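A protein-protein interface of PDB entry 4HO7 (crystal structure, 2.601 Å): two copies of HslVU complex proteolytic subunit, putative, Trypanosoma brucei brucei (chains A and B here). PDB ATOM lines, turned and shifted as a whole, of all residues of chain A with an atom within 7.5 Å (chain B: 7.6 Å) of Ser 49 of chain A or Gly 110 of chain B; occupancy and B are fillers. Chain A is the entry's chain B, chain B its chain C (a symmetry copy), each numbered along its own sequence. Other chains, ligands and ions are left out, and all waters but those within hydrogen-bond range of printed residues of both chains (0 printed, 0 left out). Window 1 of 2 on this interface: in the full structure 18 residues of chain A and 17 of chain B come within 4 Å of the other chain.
No position is printed for both chains.
Of the 16 pairs that touch across the chains among the printed residues, none has its exchanged pair printed and touching as well.
Hydrophobic or aromatic side chains of chain B that line the printed part of chain A: Ala 79.
Printed residues of chain A that touch a printed residue of chain B: Val 20, Ser 49, Thr 50, Ala 51, Asp 52, Ile 54, Ser 55 and Leu 91.
Hydrophobic or aromatic side chains of chain A that line the printed part of chain B: Val 20, Ala 51, Ile 54 and Leu 91.
Along chain A the printed residues that touch a printed residue of chain B span positions 20 to 91.
Among the printed residues, 16 pairs touch across the chains.
Among the printed residues, Asp or Glu carboxylates within 4 Å of a Lys or Arg side-chain nitrogen of the other chain: Asp 52 of chain A with Arg 83 of chain B.
The backbone NH (N) of Ala 51 of chain A sits at hydrogen-bond distance from the backbone carbonyl oxygen (O) of Gly 110 of chain B, at 3.0 Å.
OD1 of Asp 52 of chain A is in salt-bridge range of NE of Arg 83 of chain B (2.6 Å).
OG of Ser 49 of chain A lies within hydrogen-bond range of O of Gln 109 of chain B, at 3.0 Å.
The backbone NH of Glu 92 of chain A sits at hydrogen-bond distance from the side-chain carboxylate of Asp 52 of chain A (3.2 Å).
OD1 of Asp 107 of chain B lies within hydrogen-bond range of N of Gln 109 of chain B (2.9 Å).
OG of Ser 55 of chain A lies within hydrogen-bond range of O of Ala 51 of chain A (2.9 Å).
N of Asp 52 of chain A lies within hydrogen-bond range of OG of Ser 49 of chain A.
N of Asn 111 of chain B lies within hydrogen-bond range of OD1 of Asp 107 of chain B (2.9 Å).
The side-chain carboxylate (OD1) of Asp 107 of chain B sits at hydrogen-bond distance from the backbone NH (N) of Gly 110 of chain B (3.0 Å).
Among the printed residues, merely in contact across the chains: Thr 50 of chain A with Gly 110 of chain B, Ser 49 of chain A with Gly 110 of chain B, Ala 51 of chain A with Arg 83 of chain B, Ile 54 of chain A with Lys 80 of chain B, Leu 91 of chain A with Arg 83 of chain B, Ser 49 of chain A with Asn 111 of chain B, Ala 51 of chain A with Ala 79 of chain B, Leu 91 of chain A with Arg 89 of chain B, Val 20 of chain A with Asn 111 of chain B, Thr 50 of chain A with Val 112 of chain B, Asp 52 of chain A with Gln 109 of chain B, Ser 55 of chain A with Lys 80 of chain B and Ala 51 of chain A with Lys 80 of chain B.
Of the printed residues of chain B, Val 20 of chain A touches Asn 111.
Ala 47 of chain A touches none of the printed residues of chain B.
Ser 49 of chain A touches just these residues of chain B: Gln 109, Gly 110 and Asn 111.
Of the printed residues of chain B, Ala 51 of chain A touches Ala 79, Lys 80, Arg 83 and Gly 110.
Of the printed residues of chain A, Arg 89 of chain B touches Leu 91.
Gly 110 of chain B touches just these residues of chain A: Ser 49, Thr 50 and Ala 51.
Of the printed residues of chain A, Val 112 of chain B touches Thr 50.
The nearest printed residue of chain B that does not touch Val 20 of chain A is Ile 113 of chain B (4.5 Å).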
ATOM      1  N   THR A   1     -15.443   7.704  26.143  1.00  0.00           N
ATOM      2  CA  THR A   1     -15.813   8.406  24.895  1.00  0.00           C
ATOM      3  C   THR A   1     -15.152   9.760  24.810  1.00  0.00           C
ATOM      4  O   THR A   1     -14.888  10.439  25.839  1.00  0.00           O
ATOM      5  CB  THR A   1     -17.316   8.621  24.823  1.00  0.00           C
ATOM      6  OG1 THR A   1     -17.952   7.359  24.832  1.00  0.00           O
ATOM      7  CG2 THR A   1     -17.721   9.325  23.557  1.00  0.00           C
ATOM      8  N   VAL A  20     -16.815   1.259  22.685  1.00  0.00           N
ATOM      9  CA  VAL A  20     -17.852   1.053  23.607  1.00  0.00           C
ATOM     10  C   VAL A  20     -17.337   0.186  24.704  1.00  0.00           C
ATOM     11  O   VAL A  20     -16.855  -0.910  24.468  1.00  0.00           O
ATOM     12  CB  VAL A  20     -19.028   0.324  22.978  1.00  0.00           C
ATOM     13  CG1 VAL A  20     -20.120   0.080  24.033  1.00  0.00           C
ATOM     14  CG2 VAL A  20     -19.593   1.145  21.837  1.00  0.00           C
ATOM     15  N   ARG A  36     -24.108  11.372  14.146  1.00  0.00           N
ATOM     16  CA  ARG A  36     -25.252  11.211  13.240  1.00  0.00           C
ATOM     17  C   ARG A  36     -25.558  12.528  12.567  1.00  0.00           C
ATOM     18  O   ARG A  36     -25.526  13.567  13.224  1.00  0.00           O
ATOM     19  CB  ARG A  36     -26.520  10.793  13.961  1.00  0.00           C
ATOM     20  CG  ARG A  36     -26.419   9.530  14.788  1.00  0.00           C
ATOM     21  CD  ARG A  36     -26.434   8.240  13.967  1.00  0.00           C
ATOM     22  NE  ARG A  36     -26.616   7.082  14.839  1.00  0.00           N
ATOM     23  CZ  ARG A  36     -25.640   6.370  15.405  1.00  0.00           C
ATOM     24  NH1 ARG A  36     -24.368   6.639  15.183  1.00  0.00           N
ATOM     25  NH2 ARG A  36     -25.952   5.364  16.203  1.00  0.00           N
ATOM     26  N   PHE A  46     -22.435  12.013  20.226  1.00  0.00           N
ATOM     27  CA  PHE A  46     -22.956  11.640  21.511  1.00  0.00           C
ATOM     28  C   PHE A  46     -21.982  10.802  22.324  1.00  0.00           C
ATOM     29  O   PHE A  46     -21.282   9.981  21.805  1.00  0.00           O
ATOM     30  CB  PHE A  46     -24.310  10.904  21.344  1.00  0.00           C
ATOM     31  CG  PHE A  46     -24.228   9.568  20.633  1.00  0.00           C
ATOM     32  CD1 PHE A  46     -23.917   8.396  21.342  1.00  0.00           C
ATOM     33  CD2 PHE A  46     -24.527   9.468  19.255  1.00  0.00           C
ATOM     34  CE1 PHE A  46     -23.872   7.156  20.692  1.00  0.00           C
ATOM     35  CE2 PHE A  46     -24.481   8.241  18.596  1.00  0.00           C
ATOM     36  CZ  PHE A  46     -24.161   7.081  19.318  1.00  0.00           C
ATOM     37  N   ALA A  47     -21.973  11.046  23.619  1.00  0.00           N
ATOM     38  CA  ALA A  47     -21.440  10.089  24.576  1.00  0.00           C
ATOM     39  C   ALA A  47     -22.582   9.467  25.336  1.00  0.00           C
ATOM     40  O   ALA A  47     -23.431  10.179  25.889  1.00  0.00           O
ATOM     41  CB  ALA A  47     -20.544  10.798  25.553  1.00  0.00           C
ATOM     42  N   GLY A  48     -22.613   8.148  25.367  1.00  0.00           N
ATOM     43  CA  GLY A  48     -23.684   7.437  26.040  1.00  0.00           C
ATOM     44  C   GLY A  48     -24.085   6.308  25.145  1.00  0.00           C
ATOM     45  O   GLY A  48     -23.550   6.177  24.029  1.00  0.00           O
ATOM     46  N   SER A  49     -25.031   5.499  25.604  1.00  0.00           N
ATOM     47  CA  SER A  49     -25.435   4.328  24.843  1.00  0.00           C
ATOM     48  C   SER A  49     -26.206   4.707  23.573  1.00  0.00           C
ATOM     49  O   SER A  49     -26.896   5.721  23.535  1.00  0.00           O
ATOM     50  CB  SER A  49     -26.309   3.430  25.712  1.00  0.00           C
ATOM     51  OG  SER A  49     -27.614   3.975  25.804  1.00  0.00           O
ATOM     52  N   THR A  50     -26.153   3.835  22.578  1.00  0.00           N
ATOM     53  CA  THR A  50     -26.927   3.989  21.363  1.00  0.00           C
ATOM     54  C   THR A  50     -28.376   4.368  21.626  1.00  0.00           C
ATOM     55  O   THR A  50     -28.897   5.289  21.016  1.00  0.00           O
ATOM     56  CB  THR A  50     -26.938   2.674  20.622  1.00  0.00           C
ATOM     57  OG1 THR A  50     -25.579   2.261  20.478  1.00  0.00           O
ATOM     58  CG2 THR A  50     -27.598   2.778  19.230  1.00  0.00           C
ATOM     59  N   ALA A  51     -29.024   3.642  22.528  1.00  0.00           N
ATOM     60  CA  ALA A  51     -30.433   3.855  22.787  1.00  0.00           C
ATOM     61  C   ALA A  51     -30.698   5.201  23.452  1.00  0.00           C
ATOM     62  O   ALA A  51     -31.628   5.909  23.086  1.00  0.00           O
ATOM     63  CB  ALA A  51     -30.973   2.732  23.653  1.00  0.00           C
ATOM     64  N   ASP A  52     -29.917   5.522  24.475  1.00  0.00           N
ATOM     65  CA  ASP A  52     -30.149   6.760  25.222  1.00  0.00           C
ATOM     66  C   ASP A  52     -29.918   7.902  24.246  1.00  0.00           C
ATOM     67  O   ASP A  52     -30.716   8.794  24.141  1.00  0.00           O
ATOM     68  CB  ASP A  52     -29.210   6.879  26.415  1.00  0.00           C
ATOM     69  CG  ASP A  52     -29.501   5.883  27.481  1.00  0.00           C
ATOM     70  OD1 ASP A  52     -30.206   4.874  27.220  1.00  0.00           O
ATOM     71  OD2 ASP A  52     -29.019   6.110  28.616  1.00  0.00           O
ATOM     72  N   ALA A  53     -28.820   7.830  23.516  1.00  0.00           N
ATOM     73  CA  ALA A  53     -28.396   8.921  22.683  1.00  0.00           C
ATOM     74  C   ALA A  53     -29.408   9.147  21.578  1.00  0.00           C
ATOM     75  O   ALA A  53     -29.822  10.269  21.330  1.00  0.00           O
ATOM     76  CB  ALA A  53     -27.039   8.616  22.083  1.00  0.00           C
ATOM     77  N   ILE A  54     -29.828   8.074  20.939  1.00  0.00           N
ATOM     78  CA  ILE A  54     -30.804   8.181  19.878  1.00  0.00           C
ATOM     79  C   ILE A  54     -32.168   8.690  20.351  1.00  0.00           C
ATOM     80  O   ILE A  54     -32.792   9.520  19.702  1.00  0.00           O
ATOM     81  CB  ILE A  54     -30.941   6.852  19.161  1.00  0.00           C
ATOM     82  CG1 ILE A  54     -29.672   6.627  18.334  1.00  0.00           C
ATOM     83  CG2 ILE A  54     -32.174   6.850  18.280  1.00  0.00           C
ATOM     84  CD1 ILE A  54     -29.552   5.235  17.746  1.00  0.00           C
ATOM     85  N   SER A  55     -32.636   8.213  21.498  1.00  0.00           N
ATOM     86  CA  SER A  55     -33.888   8.722  22.060  1.00  0.00           C
ATOM     87  C   SER A  55     -33.819  10.228  22.194  1.00  0.00           C
ATOM     88  O   SER A  55     -34.762  10.924  21.827  1.00  0.00           O
ATOM     89  CB  SER A  55     -34.158   8.133  23.445  1.00  0.00           C
ATOM     90  OG  SER A  55     -34.366   6.742  23.411  1.00  0.00           O
ATOM     91  N   MET A  57     -31.719  12.207  20.574  1.00  0.00           N
ATOM     92  CA  MET A  57     -31.620  12.799  19.250  1.00  0.00           C
ATOM     93  C   MET A  57     -32.964  13.040  18.652  1.00  0.00           C
ATOM     94  O   MET A  57     -33.221  14.084  18.076  1.00  0.00           O
ATOM     95  CB  MET A  57     -30.796  11.944  18.299  1.00  0.00           C
ATOM     96  CG  MET A  57     -29.339  12.361  18.361  1.00  0.00           C
ATOM     97  SD  MET A  57     -28.186  11.361  17.403  1.00  0.00           S
ATOM     98  CE  MET A  57     -27.661  10.200  18.659  1.00  0.00           C
ATOM     99  N   LEU A  91     -31.960   8.506  31.586  1.00  0.00           N
ATOM    100  CA  LEU A  91     -30.889   8.313  30.583  1.00  0.00           C
ATOM    101  C   LEU A  91     -29.602   9.082  30.909  1.00  0.00           C
ATOM    102  O   LEU A  91     -29.642  10.229  31.374  1.00  0.00           O
ATOM    103  CB  LEU A  91     -31.370   8.770  29.221  1.00  0.00           C
ATOM    104  CG  LEU A  91     -32.756   8.320  28.762  1.00  0.00           C
ATOM    105  CD1 LEU A  91     -33.099   8.977  27.446  1.00  0.00           C
ATOM    106  CD2 LEU A  91     -32.830   6.814  28.624  1.00  0.00           C
ATOM    107  N   GLU A  92     -28.460   8.443  30.666  1.00  0.00           N
ATOM    108  CA  GLU A  92     -27.157   9.106  30.708  1.00  0.00           C
ATOM    109  C   GLU A  92     -26.708   9.317  29.288  1.00  0.00           C
ATOM    110  O   GLU A  92     -26.603   8.354  28.535  1.00  0.00           O
ATOM    111  CB  GLU A  92     -26.102   8.255  31.390  1.00  0.00           C
ATOM    112  CG  GLU A  92     -26.458   7.811  32.799  1.00  0.00           C
ATOM    113  CD  GLU A  92     -25.534   6.710  33.270  1.00  0.00           C
ATOM    114  OE1 GLU A  92     -26.015   5.586  33.539  1.00  0.00           O
ATOM    115  OE2 GLU A  92     -24.311   6.959  33.308  1.00  0.00           O
ATOM    116  N   ALA A  93     -26.485  10.589  28.938  1.00  0.00           N
ATOM    117  CA  ALA A  93     -25.843  10.979  27.698  1.00  0.00           C
ATOM    118  C   ALA A  93     -25.419  12.449  27.732  1.00  0.00           C
ATOM    119  O   ALA A  93     -25.804  13.233  28.596  1.00  0.00           O
ATOM    120  CB  ALA A  93     -26.743  10.728  26.491  1.00  0.00           C
ATOM    121  N   SER A  94     -24.530  12.775  26.818  1.00  0.00           N
ATOM    122  CA  SER A  94     -24.190  14.129  26.536  1.00  0.00           C
ATOM    123  C   SER A  94     -24.152  14.213  25.022  1.00  0.00           C
ATOM    124  O   SER A  94     -23.847  13.222  24.362  1.00  0.00           O
ATOM    125  CB  SER A  94     -22.835  14.458  27.125  1.00  0.00           C
ATOM    126  OG  SER A  94     -22.985  14.756  28.485  1.00  0.00           O
ATOM    127  N   ALA B  75     -33.727  -4.019  16.329  1.00  0.00           N
ATOM    128  CA  ALA B  75     -32.924  -4.132  17.522  1.00  0.00           C
ATOM    129  C   ALA B  75     -32.798  -2.782  18.191  1.00  0.00           C
ATOM    130  O   ALA B  75     -32.973  -2.630  19.406  1.00  0.00           O
ATOM    131  CB  ALA B  75     -31.565  -4.652  17.148  1.00  0.00           C
ATOM    132  N   VAL B  76     -32.529  -1.780  17.372  1.00  0.00           N
ATOM    133  CA  VAL B  76     -32.338  -0.439  17.868  1.00  0.00           C
ATOM    134  C   VAL B  76     -33.647   0.110  18.458  1.00  0.00           C
ATOM    135  O   VAL B  76     -33.618   0.839  19.459  1.00  0.00           O
ATOM    136  CB  VAL B  76     -31.786   0.475  16.742  1.00  0.00           C
ATOM    137  CG1 VAL B  76     -31.876   1.942  17.146  1.00  0.00           C
ATOM    138  CG2 VAL B  76     -30.343   0.100  16.406  1.00  0.00           C
ATOM    139  N   ALA B  79     -34.228  -1.505  21.801  1.00  0.00           N
ATOM    140  CA  ALA B  79     -33.377  -0.869  22.777  1.00  0.00           C
ATOM    141  C   ALA B  79     -33.970   0.487  23.165  1.00  0.00           C
ATOM    142  O   ALA B  79     -34.077   0.794  24.345  1.00  0.00           O
ATOM    143  CB  ALA B  79     -31.964  -0.717  22.234  1.00  0.00           C
ATOM    144  N   LYS B  80     -34.395   1.282  22.177  1.00  0.00           N
ATOM    145  CA  LYS B  80     -35.017   2.577  22.461  1.00  0.00           C
ATOM    146  C   LYS B  80     -36.210   2.453  23.409  1.00  0.00           C
ATOM    147  O   LYS B  80     -36.318   3.195  24.405  1.00  0.00           O
ATOM    148  CB  LYS B  80     -35.455   3.256  21.175  1.00  0.00           C
ATOM    149  CG  LYS B  80     -34.342   4.036  20.523  1.00  0.00           C
ATOM    150  CD  LYS B  80     -34.578   4.249  19.044  1.00  0.00           C
ATOM    151  CE  LYS B  80     -35.817   5.079  18.768  1.00  0.00           C
ATOM    152  NZ  LYS B  80     -35.918   5.233  17.297  1.00  0.00           N
ATOM    153  N   TRP B  82     -36.945  -0.070  25.363  1.00  0.00           N
ATOM    154  CA  TRP B  82     -36.503  -0.690  26.594  1.00  0.00           C
ATOM    155  C   TRP B  82     -35.978   0.382  27.572  1.00  0.00           C
ATOM    156  O   TRP B  82     -36.293   0.375  28.778  1.00  0.00           O
ATOM    157  CB  TRP B  82     -35.433  -1.727  26.211  1.00  0.00           C
ATOM    158  CG  TRP B  82     -34.852  -2.570  27.261  1.00  0.00           C
ATOM    159  CD1 TRP B  82     -35.038  -2.471  28.605  1.00  0.00           C
ATOM    160  CD2 TRP B  82     -33.910  -3.593  27.063  1.00  0.00           C
ATOM    161  NE1 TRP B  82     -34.283  -3.387  29.245  1.00  0.00           N
ATOM    162  CE2 TRP B  82     -33.566  -4.091  28.325  1.00  0.00           C
ATOM    163  CE3 TRP B  82     -33.320  -4.145  25.947  1.00  0.00           C
ATOM    164  CZ2 TRP B  82     -32.674  -5.141  28.501  1.00  0.00           C
ATOM    165  CZ3 TRP B  82     -32.424  -5.180  26.121  1.00  0.00           C
ATOM    166  CH2 TRP B  82     -32.126  -5.680  27.392  1.00  0.00           C
ATOM    167  N   ARG B  83     -35.180   1.302  27.050  1.00  0.00           N
ATOM    168  CA  ARG B  83     -34.619   2.366  27.872  1.00  0.00           C
ATOM    169  C   ARG B  83     -35.607   3.438  28.351  1.00  0.00           C
ATOM    170  O   ARG B  83     -35.334   4.151  29.319  1.00  0.00           O
ATOM    171  CB  ARG B  83     -33.489   3.030  27.098  1.00  0.00           C
ATOM    172  CG  ARG B  83     -32.314   2.106  26.902  1.00  0.00           C
ATOM    173  CD  ARG B  83     -31.653   1.801  28.235  1.00  0.00           C
ATOM    174  NE  ARG B  83     -31.033   2.991  28.801  1.00  0.00           N
ATOM    175  CZ  ARG B  83     -30.401   3.037  29.973  1.00  0.00           C
ATOM    176  NH1 ARG B  83     -30.326   1.991  30.733  1.00  0.00           N
ATOM    177  NH2 ARG B  83     -29.822   4.141  30.367  1.00  0.00           N
ATOM    178  N   ARG B  89     -37.481  -1.141  32.063  1.00  0.00           N
ATOM    179  CA  ARG B  89     -36.239  -0.763  32.681  1.00  0.00           C
ATOM    180  C   ARG B  89     -36.003  -1.461  33.994  1.00  0.00           C
ATOM    181  O   ARG B  89     -34.863  -1.565  34.423  1.00  0.00           O
ATOM    182  CB  ARG B  89     -36.181   0.725  32.879  1.00  0.00           C
ATOM    183  CG  ARG B  89     -35.603   1.389  31.665  1.00  0.00           C
ATOM    184  CD  ARG B  89     -35.104   2.751  32.029  1.00  0.00           C
ATOM    185  NE  ARG B  89     -33.841   2.703  32.758  1.00  0.00           N
ATOM    186  CZ  ARG B  89     -32.768   3.420  32.449  1.00  0.00           C
ATOM    187  NH1 ARG B  89     -32.766   4.240  31.401  1.00  0.00           N
ATOM    188  NH2 ARG B  89     -31.691   3.329  33.211  1.00  0.00           N
ATOM    189  N   GLU B 105     -26.070  -7.758  19.708  1.00  0.00           N
ATOM    190  CA  GLU B 105     -26.050  -7.888  21.137  1.00  0.00           C
ATOM    191  C   GLU B 105     -26.806  -6.671  21.602  1.00  0.00           C
ATOM    192  O   GLU B 105     -26.479  -5.550  21.188  1.00  0.00           O
ATOM    193  CB  GLU B 105     -24.600  -7.907  21.701  1.00  0.00           C
ATOM    194  CG  GLU B 105     -24.460  -7.623  23.195  1.00  0.00           C
ATOM    195  CD  GLU B 105     -23.026  -7.608  23.705  1.00  0.00           C
ATOM    196  OE1 GLU B 105     -22.106  -7.849  22.866  1.00  0.00           O
ATOM    197  OE2 GLU B 105     -22.813  -7.300  24.927  1.00  0.00           O
ATOM    198  N   ILE B 106     -27.819  -6.888  22.444  1.00  0.00           N
ATOM    199  CA  ILE B 106     -28.525  -5.791  23.072  1.00  0.00           C
ATOM    200  C   ILE B 106     -28.591  -5.970  24.583  1.00  0.00           C
ATOM    201  O   ILE B 106     -28.933  -7.034  25.068  1.00  0.00           O
ATOM    202  CB  ILE B 106     -29.950  -5.699  22.563  1.00  0.00           C
ATOM    203  CG1 ILE B 106     -30.001  -5.976  21.076  1.00  0.00           C
ATOM    204  CG2 ILE B 106     -30.522  -4.322  22.832  1.00  0.00           C
ATOM    205  CD1 ILE B 106     -31.410  -6.231  20.587  1.00  0.00           C
ATOM    206  N   ASP B 107     -28.274  -4.912  25.330  1.00  0.00           N
ATOM    207  CA  ASP B 107     -28.309  -4.940  26.792  1.00  0.00           C
ATOM    208  C   ASP B 107     -29.210  -3.862  27.346  1.00  0.00           C
ATOM    209  O   ASP B 107     -29.853  -3.083  26.608  1.00  0.00           O
ATOM    210  CB  ASP B 107     -26.882  -4.857  27.380  1.00  0.00           C
ATOM    211  CG  ASP B 107     -26.227  -3.531  27.139  1.00  0.00           C
ATOM    212  OD1 ASP B 107     -26.919  -2.509  26.957  1.00  0.00           O
ATOM    213  OD2 ASP B 107     -24.990  -3.494  27.145  1.00  0.00           O
ATOM    214  N   GLY B 108     -29.275  -3.843  28.675  1.00  0.00           N
ATOM    215  CA  GLY B 108     -30.191  -2.972  29.382  1.00  0.00           C
ATOM    216  C   GLY B 108     -29.581  -1.629  29.623  1.00  0.00           C
ATOM    217  O   GLY B 108     -30.240  -0.761  30.147  1.00  0.00           O
ATOM    218  N   GLN B 109     -28.319  -1.438  29.250  1.00  0.00           N
ATOM    219  CA  GLN B 109     -27.725  -0.091  29.248  1.00  0.00           C
ATOM    220  C   GLN B 109     -28.101   0.623  27.961  1.00  0.00           C
ATOM    221  O   GLN B 109     -27.801   1.785  27.784  1.00  0.00           O
ATOM    222  CB  GLN B 109     -26.179  -0.182  29.377  1.00  0.00           C
ATOM    223  CG  GLN B 109     -25.610   0.104  30.774  1.00  0.00           C
ATOM    224  CD  GLN B 109     -26.442  -0.519  31.914  1.00  0.00           C
ATOM    225  OE1 GLN B 109     -27.020   0.203  32.757  1.00  0.00           O
ATOM    226  NE2 GLN B 109     -26.586  -1.859  31.881  1.00  0.00           N
ATOM    227  N   GLY B 110     -28.703  -0.099  27.033  1.00  0.00           N
ATOM    228  CA  GLY B 110     -29.077   0.468  25.757  1.00  0.00           C
ATOM    229  C   GLY B 110     -27.996   0.377  24.676  1.00  0.00           C
ATOM    230  O   GLY B 110     -28.048   1.085  23.670  1.00  0.00           O
ATOM    231  N   ASN B 111     -27.002  -0.465  24.867  1.00  0.00           N
ATOM    232  CA  ASN B 111     -26.006  -0.658  23.821  1.00  0.00           C
ATOM    233  C   ASN B 111     -26.544  -1.609  22.787  1.00  0.00           C
ATOM    234  O   ASN B 111     -27.324  -2.515  23.092  1.00  0.00           O
ATOM    235  CB  ASN B 111     -24.741  -1.224  24.411  1.00  0.00           C
ATOM    236  CG  ASN B 111     -24.076  -0.268  25.371  1.00  0.00           C
ATOM    237  OD1 ASN B 111     -23.730   0.847  24.986  1.00  0.00           O
ATOM    238  ND2 ASN B 111     -23.898  -0.694  26.637  1.00  0.00           N
ATOM    239  N   VAL B 112     -26.205  -1.355  21.551  1.00  0.00           N
ATOM    240  CA  VAL B 112     -26.550  -2.263  20.470  1.00  0.00           C
ATOM    241  C   VAL B 112     -25.249  -2.484  19.707  1.00  0.00           C
ATOM    242  O   VAL B 112     -24.745  -1.577  19.070  1.00  0.00           O
ATOM    243  CB  VAL B 112     -27.619  -1.672  19.540  1.00  0.00           C
ATOM    244  CG1 VAL B 112     -27.914  -2.633  18.389  1.00  0.00           C
ATOM    245  CG2 VAL B 112     -28.882  -1.402  20.337  1.00  0.00           C
ATOM    246  N   ILE B 113     -24.735  -3.701  19.801  1.00  0.00           N
ATOM    247  CA  ILE B 113     -23.415  -4.019  19.418  1.00  0.00           C
ATOM    248  C   ILE B 113     -23.454  -5.067  18.351  1.00  0.00           C
ATOM    249  O   ILE B 113     -24.071  -6.094  18.493  1.00  0.00           O
ATOM    250  CB  ILE B 113     -22.713  -4.570  20.632  1.00  0.00           C
ATOM    251  CG1 ILE B 113     -22.376  -3.393  21.546  1.00  0.00           C
ATOM    252  CG2 ILE B 113     -21.451  -5.356  20.302  1.00  0.00           C
ATOM    253  CD1 ILE B 113     -22.143  -3.833  22.961  1.00  0.00           C
